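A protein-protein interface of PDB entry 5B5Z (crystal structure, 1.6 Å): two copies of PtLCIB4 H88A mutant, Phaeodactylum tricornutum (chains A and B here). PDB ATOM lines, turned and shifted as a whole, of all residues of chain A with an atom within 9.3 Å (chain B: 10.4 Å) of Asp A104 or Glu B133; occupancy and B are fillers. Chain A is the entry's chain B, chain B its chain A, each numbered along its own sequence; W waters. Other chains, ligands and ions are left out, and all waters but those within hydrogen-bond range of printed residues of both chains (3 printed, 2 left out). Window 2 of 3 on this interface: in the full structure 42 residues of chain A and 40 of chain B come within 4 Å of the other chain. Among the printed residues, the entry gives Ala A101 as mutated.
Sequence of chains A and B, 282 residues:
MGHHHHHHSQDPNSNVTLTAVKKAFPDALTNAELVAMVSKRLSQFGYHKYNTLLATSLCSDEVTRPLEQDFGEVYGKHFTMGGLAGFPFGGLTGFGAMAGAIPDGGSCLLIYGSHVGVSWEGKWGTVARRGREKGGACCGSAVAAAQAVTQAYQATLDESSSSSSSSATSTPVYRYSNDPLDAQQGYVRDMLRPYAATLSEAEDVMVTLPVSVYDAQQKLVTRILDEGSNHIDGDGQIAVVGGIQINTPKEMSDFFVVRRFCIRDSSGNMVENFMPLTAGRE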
ATOM      1  N   TYR A  50      -0.346  18.495 -18.914  1.00  0.00           N
ATOM      2  CA  TYR A  50      -0.936  19.731 -18.416  1.00  0.00           C
ATOM      3  C   TYR A  50      -0.196  20.971 -18.907  1.00  0.00           C
ATOM      4  O   TYR A  50      -0.789  22.042 -18.993  1.00  0.00           O
ATOM      5  CB  TYR A  50      -0.997  19.724 -16.879  1.00  0.00           C
ATOM      6  CG  TYR A  50       0.286  20.121 -16.194  1.00  0.00           C
ATOM      7  CD1 TYR A  50       1.346  19.234 -16.101  1.00  0.00           C
ATOM      8  CD2 TYR A  50       0.432  21.384 -15.620  1.00  0.00           C
ATOM      9  CE1 TYR A  50       2.520  19.594 -15.474  1.00  0.00           C
ATOM     10  CE2 TYR A  50       1.602  21.752 -14.991  1.00  0.00           C
ATOM     11  CZ  TYR A  50       2.644  20.843 -14.916  1.00  0.00           C
ATOM     12  OH  TYR A  50       3.817  21.186 -14.291  1.00  0.00           O
ATOM     13  N   ASN A  51       1.084  20.833 -19.253  1.00  0.00           N
ATOM     14  CA  ASN A  51       1.915  22.005 -19.519  1.00  0.00           C
ATOM     15  C   ASN A  51       2.515  22.050 -20.930  1.00  0.00           C
ATOM     16  O   ASN A  51       3.391  22.870 -21.208  1.00  0.00           O
ATOM     17  CB  ASN A  51       3.046  22.096 -18.486  1.00  0.00           C
ATOM     18  CG  ASN A  51       4.064  20.970 -18.623  1.00  0.00           C
ATOM     19  OD1 ASN A  51       3.765  19.904 -19.157  1.00  0.00           O
ATOM     20  ND2 ASN A  51       5.271  21.211 -18.139  1.00  0.00           N
ATOM     21  N   THR A  52       2.039  21.175 -21.804  1.00  0.00           N
ATOM     22  CA  THR A  52       2.523  21.141 -23.187  1.00  0.00           C
ATOM     23  C   THR A  52       1.418  21.476 -24.170  1.00  0.00           C
ATOM     24  O   THR A  52       0.333  20.912 -24.089  1.00  0.00           O
ATOM     25  CB  THR A  52       3.073  19.764 -23.566  1.00  0.00           C
ATOM     26  OG1 THR A  52       4.122  19.402 -22.662  1.00  0.00           O
ATOM     27  CG2 THR A  52       3.624  19.792 -24.990  1.00  0.00           C
ATOM     28  N   LEU A  53       1.706  22.386 -25.102  1.00  0.00           N
ATOM     29  CA  LEU A  53       0.787  22.705 -26.189  1.00  0.00           C
ATOM     30  C   LEU A  53       1.302  22.019 -27.448  1.00  0.00           C
ATOM     31  O   LEU A  53       2.443  22.226 -27.836  1.00  0.00           O
ATOM     32  CB  LEU A  53       0.678  24.213 -26.405  1.00  0.00           C
ATOM     33  CG  LEU A  53      -0.180  24.592 -27.611  1.00  0.00           C
ATOM     34  CD1 LEU A  53      -1.636  24.183 -27.416  1.00  0.00           C
ATOM     35  CD2 LEU A  53      -0.079  26.080 -27.842  1.00  0.00           C
ATOM     36  N   ALA A  99       2.105  30.379 -29.587  1.00  0.00           N
ATOM     37  CA  ALA A  99       2.908  30.740 -28.420  1.00  0.00           C
ATOM     38  C   ALA A  99       2.046  31.379 -27.340  1.00  0.00           C
ATOM     39  O   ALA A  99       2.219  31.120 -26.146  1.00  0.00           O
ATOM     40  CB  ALA A  99       4.032  31.680 -28.826  1.00  0.00           C
ATOM     41  N   GLY A 100       1.094  32.197 -27.770  1.00  0.00           N
ATOM     42  CA  GLY A 100       0.183  32.849 -26.852  1.00  0.00           C
ATOM     43  C   GLY A 100      -0.809  31.931 -26.164  1.00  0.00           C
ATOM     44  O   GLY A 100      -1.559  32.391 -25.299  1.00  0.00           O
ATOM     45  N   ALA A 101      -0.824  30.653 -26.537  1.00  0.00           N
ATOM     46  CA  ALA A 101      -1.727  29.671 -25.944  1.00  0.00           C
ATOM     47  C   ALA A 101      -0.994  28.646 -25.090  1.00  0.00           C
ATOM     48  O   ALA A 101      -1.612  27.734 -24.555  1.00  0.00           O
ATOM     49  CB  ALA A 101      -2.512  28.953 -27.025  1.00  0.00           C
ATOM     50  N   ILE A 102       0.325  28.757 -25.015  1.00  0.00           N
ATOM     51  CA  ILE A 102       1.106  27.802 -24.239  1.00  0.00           C
ATOM     52  C   ILE A 102       0.752  27.968 -22.770  1.00  0.00           C
ATOM     53  O   ILE A 102       0.623  29.098 -22.304  1.00  0.00           O
ATOM     54  CB  ILE A 102       2.613  28.012 -24.450  1.00  0.00           C
ATOM     55  CG1 ILE A 102       2.988  27.680 -25.894  1.00  0.00           C
ATOM     56  CG2 ILE A 102       3.418  27.127 -23.514  1.00  0.00           C
ATOM     57  CD1 ILE A 102       4.414  28.026 -26.243  1.00  0.00           C
ATOM     58  N   PRO A 103       0.541  26.850 -22.055  1.00  0.00           N
ATOM     59  CA  PRO A 103       0.287  26.942 -20.608  1.00  0.00           C
ATOM     60  C   PRO A 103       1.365  27.749 -19.894  1.00  0.00           C
ATOM     61  O   PRO A 103       2.533  27.698 -20.290  1.00  0.00           O
ATOM     62  CB  PRO A 103       0.304  25.484 -20.167  1.00  0.00           C
ATOM     63  CG  PRO A 103      -0.226  24.746 -21.363  1.00  0.00           C
ATOM     64  CD  PRO A 103       0.366  25.471 -22.550  1.00  0.00           C
ATOM     65  N   ASP A 104       0.978  28.482 -18.854  1.00  0.00           N
ATOM     66  CA  ASP A 104       1.936  29.293 -18.103  1.00  0.00           C
ATOM     67  C   ASP A 104       3.100  28.446 -17.592  1.00  0.00           C
ATOM     68  O   ASP A 104       2.895  27.410 -16.964  1.00  0.00           O
ATOM     69  CB  ASP A 104       1.242  29.999 -16.928  1.00  0.00           C
ATOM     70  CG  ASP A 104       0.237  31.047 -17.385  1.00  0.00           C
ATOM     71  OD1 ASP A 104       0.374  31.548 -18.523  1.00  0.00           O
ATOM     72  OD2 ASP A 104      -0.681  31.381 -16.599  1.00  0.00           O
ATOM     73  N   GLY A 105       4.321  28.878 -17.895  1.00  0.00           N
ATOM     74  CA  GLY A 105       5.511  28.145 -17.499  1.00  0.00           C
ATOM     75  C   GLY A 105       5.744  26.864 -18.287  1.00  0.00           C
ATOM     76  O   GLY A 105       6.695  26.127 -18.008  1.00  0.00           O
ATOM     77  N   GLY A 106       4.878  26.597 -19.269  1.00  0.00           N
ATOM     78  CA  GLY A 106       4.964  25.385 -20.072  1.00  0.00           C
ATOM     79  C   GLY A 106       5.687  25.568 -21.398  1.00  0.00           C
ATOM     80  O   GLY A 106       6.382  26.554 -21.604  1.00  0.00           O
ATOM     81  N   SER A 107       5.523  24.610 -22.303  1.00  0.00           N
ATOM     82  CA  SER A 107       6.267  24.619 -23.563  1.00  0.00           C
ATOM     83  C   SER A 107       5.401  24.152 -24.716  1.00  0.00           C
ATOM     84  O   SER A 107       4.284  23.683 -24.510  1.00  0.00           O
ATOM     85  CB  SER A 107       7.503  23.727 -23.468  1.00  0.00           C
ATOM     86  OG  SER A 107       8.421  24.234 -22.512  1.00  0.00           O
ATOM     87  N   ASP A 233       7.772  32.663 -23.599  1.00  0.00           N
ATOM     88  CA  ASP A 233       8.087  33.252 -22.302  1.00  0.00           C
ATOM     89  C   ASP A 233       9.275  32.572 -21.610  1.00  0.00           C
ATOM     90  O   ASP A 233       9.309  31.353 -21.475  1.00  0.00           O
ATOM     91  CB  ASP A 233       6.856  33.202 -21.397  1.00  0.00           C
ATOM     92  CG  ASP A 233       5.722  34.078 -21.904  1.00  0.00           C
ATOM     93  OD1 ASP A 233       5.947  35.295 -22.083  1.00  0.00           O
ATOM     94  OD2 ASP A 233       4.602  33.560 -22.109  1.00  0.00           O
ATOM     95  N   ASP A 235      11.097  30.857 -19.356  1.00  0.00           N
ATOM     96  CA  ASP A 235      11.407  29.465 -19.051  1.00  0.00           C
ATOM     97  C   ASP A 235      10.897  28.542 -20.154  1.00  0.00           C
ATOM     98  O   ASP A 235      11.419  27.440 -20.353  1.00  0.00           O
ATOM     99  CB  ASP A 235      10.800  29.065 -17.704  1.00  0.00           C
ATOM    100  N   GLY A 236       9.877  29.010 -20.870  1.00  0.00           N
ATOM    101  CA  GLY A 236       9.228  28.226 -21.904  1.00  0.00           C
ATOM    102  C   GLY A 236      10.158  27.790 -23.018  1.00  0.00           C
ATOM    103  O   GLY A 236      11.105  28.490 -23.373  1.00  0.00           O
ATOM    104  N   GLN A 237       9.879  26.619 -23.574  1.00  0.00           N
ATOM    105  CA  GLN A 237      10.689  26.084 -24.654  1.00  0.00           C
ATOM    106  C   GLN A 237       9.830  25.702 -25.839  1.00  0.00           C
ATOM    107  O   GLN A 237       8.599  25.690 -25.751  1.00  0.00           O
ATOM    108  CB  GLN A 237      11.459  24.852 -24.195  1.00  0.00           C
ATOM    109  CG  GLN A 237      12.445  25.106 -23.095  1.00  0.00           C
ATOM    110  CD  GLN A 237      13.039  23.827 -22.580  1.00  0.00           C
ATOM    111  OE1 GLN A 237      12.398  22.772 -22.622  1.00  0.00           O
ATOM    112  NE2 GLN A 237      14.276  23.901 -22.099  1.00  0.00           N
ATOM    113  N   SER B 119     -16.496  34.358 -22.773  1.00  0.00           N
ATOM    114  CA  SER B 119     -15.894  34.006 -21.490  1.00  0.00           C
ATOM    115  C   SER B 119     -16.942  33.599 -20.463  1.00  0.00           C
ATOM    116  O   SER B 119     -18.142  33.665 -20.718  1.00  0.00           O
ATOM    117  CB  SER B 119     -15.070  35.169 -20.940  1.00  0.00           C
ATOM    118  OG  SER B 119     -15.907  36.237 -20.526  1.00  0.00           O
ATOM    119  N   TRP B 120     -16.470  33.185 -19.293  1.00  0.00           N
ATOM    120  CA  TRP B 120     -17.363  32.841 -18.199  1.00  0.00           C
ATOM    121  C   TRP B 120     -18.177  34.064 -17.769  1.00  0.00           C
ATOM    122  O   TRP B 120     -19.269  33.916 -17.224  1.00  0.00           O
ATOM    123  CB  TRP B 120     -16.574  32.270 -17.013  1.00  0.00           C
ATOM    124  CG  TRP B 120     -15.669  33.270 -16.357  1.00  0.00           C
ATOM    125  CD1 TRP B 120     -14.494  33.765 -16.849  1.00  0.00           C
ATOM    126  CD2 TRP B 120     -15.867  33.903 -15.083  1.00  0.00           C
ATOM    127  NE1 TRP B 120     -13.950  34.663 -15.962  1.00  0.00           N
ATOM    128  CE2 TRP B 120     -14.771  34.764 -14.870  1.00  0.00           C
ATOM    129  CE3 TRP B 120     -16.860  33.821 -14.103  1.00  0.00           C
ATOM    130  CZ2 TRP B 120     -14.643  35.540 -13.714  1.00  0.00           C
ATOM    131  CZ3 TRP B 120     -16.732  34.595 -12.956  1.00  0.00           C
ATOM    132  CH2 TRP B 120     -15.633  35.442 -12.773  1.00  0.00           C
ATOM    133  N   GLU B 121     -17.661  35.263 -18.041  1.00  0.00           N
ATOM    134  CA  GLU B 121     -18.372  36.509 -17.720  1.00  0.00           C
ATOM    135  C   GLU B 121     -19.246  37.030 -18.862  1.00  0.00           C
ATOM    136  O   GLU B 121     -19.794  38.135 -18.765  1.00  0.00           O
ATOM    137  CB  GLU B 121     -17.391  37.623 -17.350  1.00  0.00           C
ATOM    138  CG  GLU B 121     -16.577  37.416 -16.090  1.00  0.00           C
ATOM    139  CD  GLU B 121     -15.275  38.212 -16.130  1.00  0.00           C
ATOM    140  OE1 GLU B 121     -15.298  39.366 -16.610  1.00  0.00           O
ATOM    141  OE2 GLU B 121     -14.225  37.691 -15.699  1.00  0.00           O
ATOM    142  N   THR B 126     -12.880  36.509 -26.401  1.00  0.00           N
ATOM    143  CA  THR B 126     -11.899  35.908 -25.512  1.00  0.00           C
ATOM    144  C   THR B 126     -12.483  34.668 -24.846  1.00  0.00           C
ATOM    145  O   THR B 126     -13.699  34.550 -24.669  1.00  0.00           O
ATOM    146  CB  THR B 126     -11.410  36.912 -24.434  1.00  0.00           C
ATOM    147  OG1 THR B 126     -10.334  36.330 -23.685  1.00  0.00           O
ATOM    148  CG2 THR B 126     -12.543  37.318 -23.482  1.00  0.00           C
ATOM    149  N   VAL B 127     -11.616  33.729 -24.490  1.00  0.00           N
ATOM    150  CA  VAL B 127     -12.058  32.546 -23.766  1.00  0.00           C
ATOM    151  C   VAL B 127     -10.868  31.955 -23.016  1.00  0.00           C
ATOM    152  O   VAL B 127      -9.722  32.076 -23.450  1.00  0.00           O
ATOM    153  CB  VAL B 127     -12.710  31.499 -24.708  1.00  0.00           C
ATOM    154  CG1 VAL B 127     -11.672  30.882 -25.649  1.00  0.00           C
ATOM    155  CG2 VAL B 127     -13.447  30.435 -23.899  1.00  0.00           C
ATOM    156  N   ALA B 128     -11.142  31.384 -21.850  1.00  0.00           N
ATOM    157  CA  ALA B 128     -10.089  30.819 -21.030  1.00  0.00           C
ATOM    158  C   ALA B 128      -9.413  29.686 -21.775  1.00  0.00           C
ATOM    159  O   ALA B 128     -10.072  28.911 -22.470  1.00  0.00           O
ATOM    160  CB  ALA B 128     -10.651  30.329 -19.691  1.00  0.00           C
ATOM    161  N   ARG B 129      -8.094  29.617 -21.645  1.00  0.00           N
ATOM    162  CA  ARG B 129      -7.303  28.564 -22.268  1.00  0.00           C
ATOM    163  C   ARG B 129      -6.606  27.705 -21.217  1.00  0.00           C
ATOM    164  O   ARG B 129      -6.195  28.208 -20.173  1.00  0.00           O
ATOM    165  CB  ARG B 129      -6.278  29.171 -23.226  1.00  0.00           C
ATOM    166  CG  ARG B 129      -6.905  29.814 -24.457  1.00  0.00           C
ATOM    167  CD  ARG B 129      -5.845  30.313 -25.426  1.00  0.00           C
ATOM    168  NE  ARG B 129      -6.442  31.111 -26.498  1.00  0.00           N
ATOM    169  CZ  ARG B 129      -6.783  30.628 -27.690  1.00  0.00           C
ATOM    170  NH1 ARG B 129      -6.571  29.356 -27.970  1.00  0.00           N
ATOM    171  NH2 ARG B 129      -7.329  31.421 -28.601  1.00  0.00           N
ATOM    172  N   ARG B 130      -6.477  26.414 -21.506  1.00  0.00           N
ATOM    173  CA  ARG B 130      -5.887  25.456 -20.580  1.00  0.00           C
ATOM    174  C   ARG B 130      -4.532  25.932 -20.056  1.00  0.00           C
ATOM    175  O   ARG B 130      -3.674  26.370 -20.822  1.00  0.00           O
ATOM    176  CB  ARG B 130      -5.748  24.086 -21.259  1.00  0.00           C
ATOM    177  CG  ARG B 130      -4.964  23.062 -20.452  1.00  0.00           C
ATOM    178  CD  ARG B 130      -4.949  21.692 -21.118  1.00  0.00           C
ATOM    179  NE  ARG B 130      -4.370  21.701 -22.465  1.00  0.00           N
ATOM    180  CZ  ARG B 130      -3.066  21.664 -22.720  1.00  0.00           C
ATOM    181  NH1 ARG B 130      -2.197  21.639 -21.725  1.00  0.00           N
ATOM    182  NH2 ARG B 130      -2.628  21.660 -23.974  1.00  0.00           N
ATOM    183  N   GLY B 131      -4.360  25.878 -18.739  1.00  0.00           N
ATOM    184  CA  GLY B 131      -3.088  26.211 -18.122  1.00  0.00           C
ATOM    185  C   GLY B 131      -2.694  27.674 -18.159  1.00  0.00           C
ATOM    186  O   GLY B 131      -1.559  28.019 -17.826  1.00  0.00           O
ATOM    187  N   ARG B 132      -3.624  28.542 -18.544  1.00  0.00           N
ATOM    188  CA  ARG B 132      -3.329  29.968 -18.639  1.00  0.00           C
ATOM    189  C   ARG B 132      -4.217  30.814 -17.752  1.00  0.00           C
ATOM    190  O   ARG B 132      -5.420  30.583 -17.661  1.00  0.00           O
ATOM    191  CB  ARG B 132      -3.475  30.448 -20.076  1.00  0.00           C
ATOM    192  CG  ARG B 132      -2.389  29.945 -20.989  1.00  0.00           C
ATOM    193  CD  ARG B 132      -2.337  30.790 -22.233  1.00  0.00           C
ATOM    194  NE  ARG B 132      -0.955  31.036 -22.601  1.00  0.00           N
ATOM    195  CZ  ARG B 132      -0.351  32.212 -22.504  1.00  0.00           C
ATOM    196  NH1 ARG B 132      -1.018  33.271 -22.078  1.00  0.00           N
ATOM    197  NH2 ARG B 132       0.915  32.324 -22.864  1.00  0.00           N
ATOM    198  N   GLU B 133      -3.607  31.805 -17.120  1.00  0.00           N
ATOM    199  CA  GLU B 133      -4.328  32.787 -16.332  1.00  0.00           C
ATOM    200  C   GLU B 133      -5.104  33.721 -17.257  1.00  0.00           C
ATOM    201  O   GLU B 133      -6.270  34.028 -17.008  1.00  0.00           O
ATOM    202  CB  GLU B 133      -3.352  33.573 -15.452  1.00  0.00           C
ATOM    203  CG  GLU B 133      -3.917  34.811 -14.779  1.00  0.00           C
ATOM    204  CD  GLU B 133      -2.829  35.692 -14.192  1.00  0.00           C
ATOM    205  OE1 GLU B 133      -2.609  36.814 -14.705  1.00  0.00           O
ATOM    206  OE2 GLU B 133      -2.179  35.251 -13.220  1.00  0.00           O
ATOM    207  N   LYS B 134      -4.449  34.147 -18.335  1.00  0.00           N
ATOM    208  CA  LYS B 134      -5.069  35.009 -19.346  1.00  0.00           C
ATOM    209  C   LYS B 134      -5.243  34.269 -20.678  1.00  0.00           C
ATOM    210  O   LYS B 134      -4.288  33.697 -21.213  1.00  0.00           O
ATOM    211  CB  LYS B 134      -4.238  36.274 -19.556  1.00  0.00           C
ATOM    212  CG  LYS B 134      -4.300  37.266 -18.402  1.00  0.00           C
ATOM    213  CD  LYS B 134      -3.311  38.409 -18.599  1.00  0.00           C
ATOM    214  CE  LYS B 134      -2.502  38.679 -17.340  1.00  0.00           C
ATOM    215  NZ  LYS B 134      -1.037  38.693 -17.611  1.00  0.00           N
ATOM    216  N   GLY B 135      -6.461  34.293 -21.211  1.00  0.00           N
ATOM    217  CA  GLY B 135      -6.784  33.541 -22.412  1.00  0.00           C
ATOM    218  C   GLY B 135      -6.386  34.223 -23.706  1.00  0.00           C
ATOM    219  O   GLY B 135      -6.094  33.565 -24.703  1.00  0.00           O
ATOM    220  N   GLY B 136      -6.374  35.550 -23.700  1.00  0.00           N
ATOM    221  CA  GLY B 136      -6.038  36.291 -24.897  1.00  0.00           C
ATOM    222  C   GLY B 136      -7.176  36.246 -25.898  1.00  0.00           C
ATOM    223  O   GLY B 136      -8.240  35.693 -25.613  1.00  0.00           O
HETATM  224  O   HOH W   1       0.040  26.080 -16.369  1.00  0.00           O
HETATM  225  O   HOH W   2      -3.524  26.312 -23.513  1.00  0.00           O
HETATM  226  O   HOH W   3       3.872  31.874 -23.863  1.00  0.00           O
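Water W3 lies within hydrogen-bond range of OD2 of Asp A233, O of Ala A99 and NH2 of Arg B132.
Water W2 lies within hydrogen-bond range of the backbone carbonyl oxygen of Ala A101 (2.6 Å) and the backbone carbonyl oxygen of Arg B130 (2.7 Å).
Water W1 bridges O of Gly B131 (2.9 Å) and O of Asp A104 (3.2 Å).
The guanidinium group (NH1) of Arg B132 lies within hydrogen-bond range of the backbone carbonyl oxygen (O) of Lys B134, at 3.4 Å.
OE1 of Glu B133 is in salt-bridge range of NZ of Lys B134, at 3.8 Å.
O of Gly B135 lies within hydrogen-bond range of NE of Arg B129 (3.1 Å).
No position is printed for both chains.
The side-chain carboxylate (OD2) of Asp A233 is in salt-bridge range of the guanidinium group (NH2) of Arg B132 (3.96 Å).
The backbone carbonyl oxygen (O) of Thr A52 sits at hydrogen-bond distance from the guanidinium group (NH2) of Arg B130, 3.1 Å away.
The backbone NH (N) of Asp A104 lies within hydrogen-bond range of the backbone carbonyl oxygen (O) of Gly B131 (2.8 Å).
The guanidinium group (NE) of Arg B132 lies within hydrogen-bond range of the backbone carbonyl oxygen (O) of Ile A102 (2.5 Å).
The guanidinium group (NE) of Arg B132 lies close to the backbone carbonyl oxygen (O) of Gly A100 (3.1 Å).
The side-chain carboxylate (OD2) of Asp A104 lies within hydrogen-bond range of the backbone NH (N) of Glu B133 (3.0 Å).
The backbone carbonyl oxygen (O) of Tyr A50 sits at hydrogen-bond distance from the guanidinium group (NH1) of Arg B130 (3.1 Å).
Printed residues of chain A that touch a printed residue of chain B: Tyr A50, Thr A52, Ala A99, Gly A100, Ala A101, Ile A102, Pro A103, Asp A104 and Asp A233.
Among the printed residues, Asp or Glu carboxylates within 4 Å of a Lys or Arg side-chain nitrogen of the other chain: Asp A233 with Arg B132 (3.96 Å).
Arg B132 touches Ala A99 (NH2 to O, 3.7 Å).
CD of Arg B129 touches CB of Ala A101, 3.9 Å away.
Ala A101 touches Arg B132.
Pro A103 touches Arg B130.
Pro A103 touches Gly B131 (CA to O, 3.5 Å).
Arg B132 touches Asp A104.
Of the printed residues of chain A, Glu B133 touches Asp A104 (3.0 Å).
No residue of chain B comes within 4 Å of Gly A106.
No residue of chain A comes within 4 Å of Lys B134.
Printed residues of chain B within 4 Å of Tyr A50: Arg B130.
Of the printed residues of chain B, Gly A100 touches Arg B132 (3.1 Å).
Printed residues of chain A within 4 Å of Arg B130: Tyr A50, Thr A52 and Pro A103.
Of the printed residues of chain B, Ala A101 touches Arg B129 and Arg B132.
Printed residues of chain B within 4 Å of Asp A233: Arg B132 (3.96 Å).
Leu A53 touches none of the printed residues of chain B.
Ser A107 touches none of the printed residues of chain B.
The nearest residue of chain B that does not touch Asp A104 is Lys B134 (5.0 Å).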
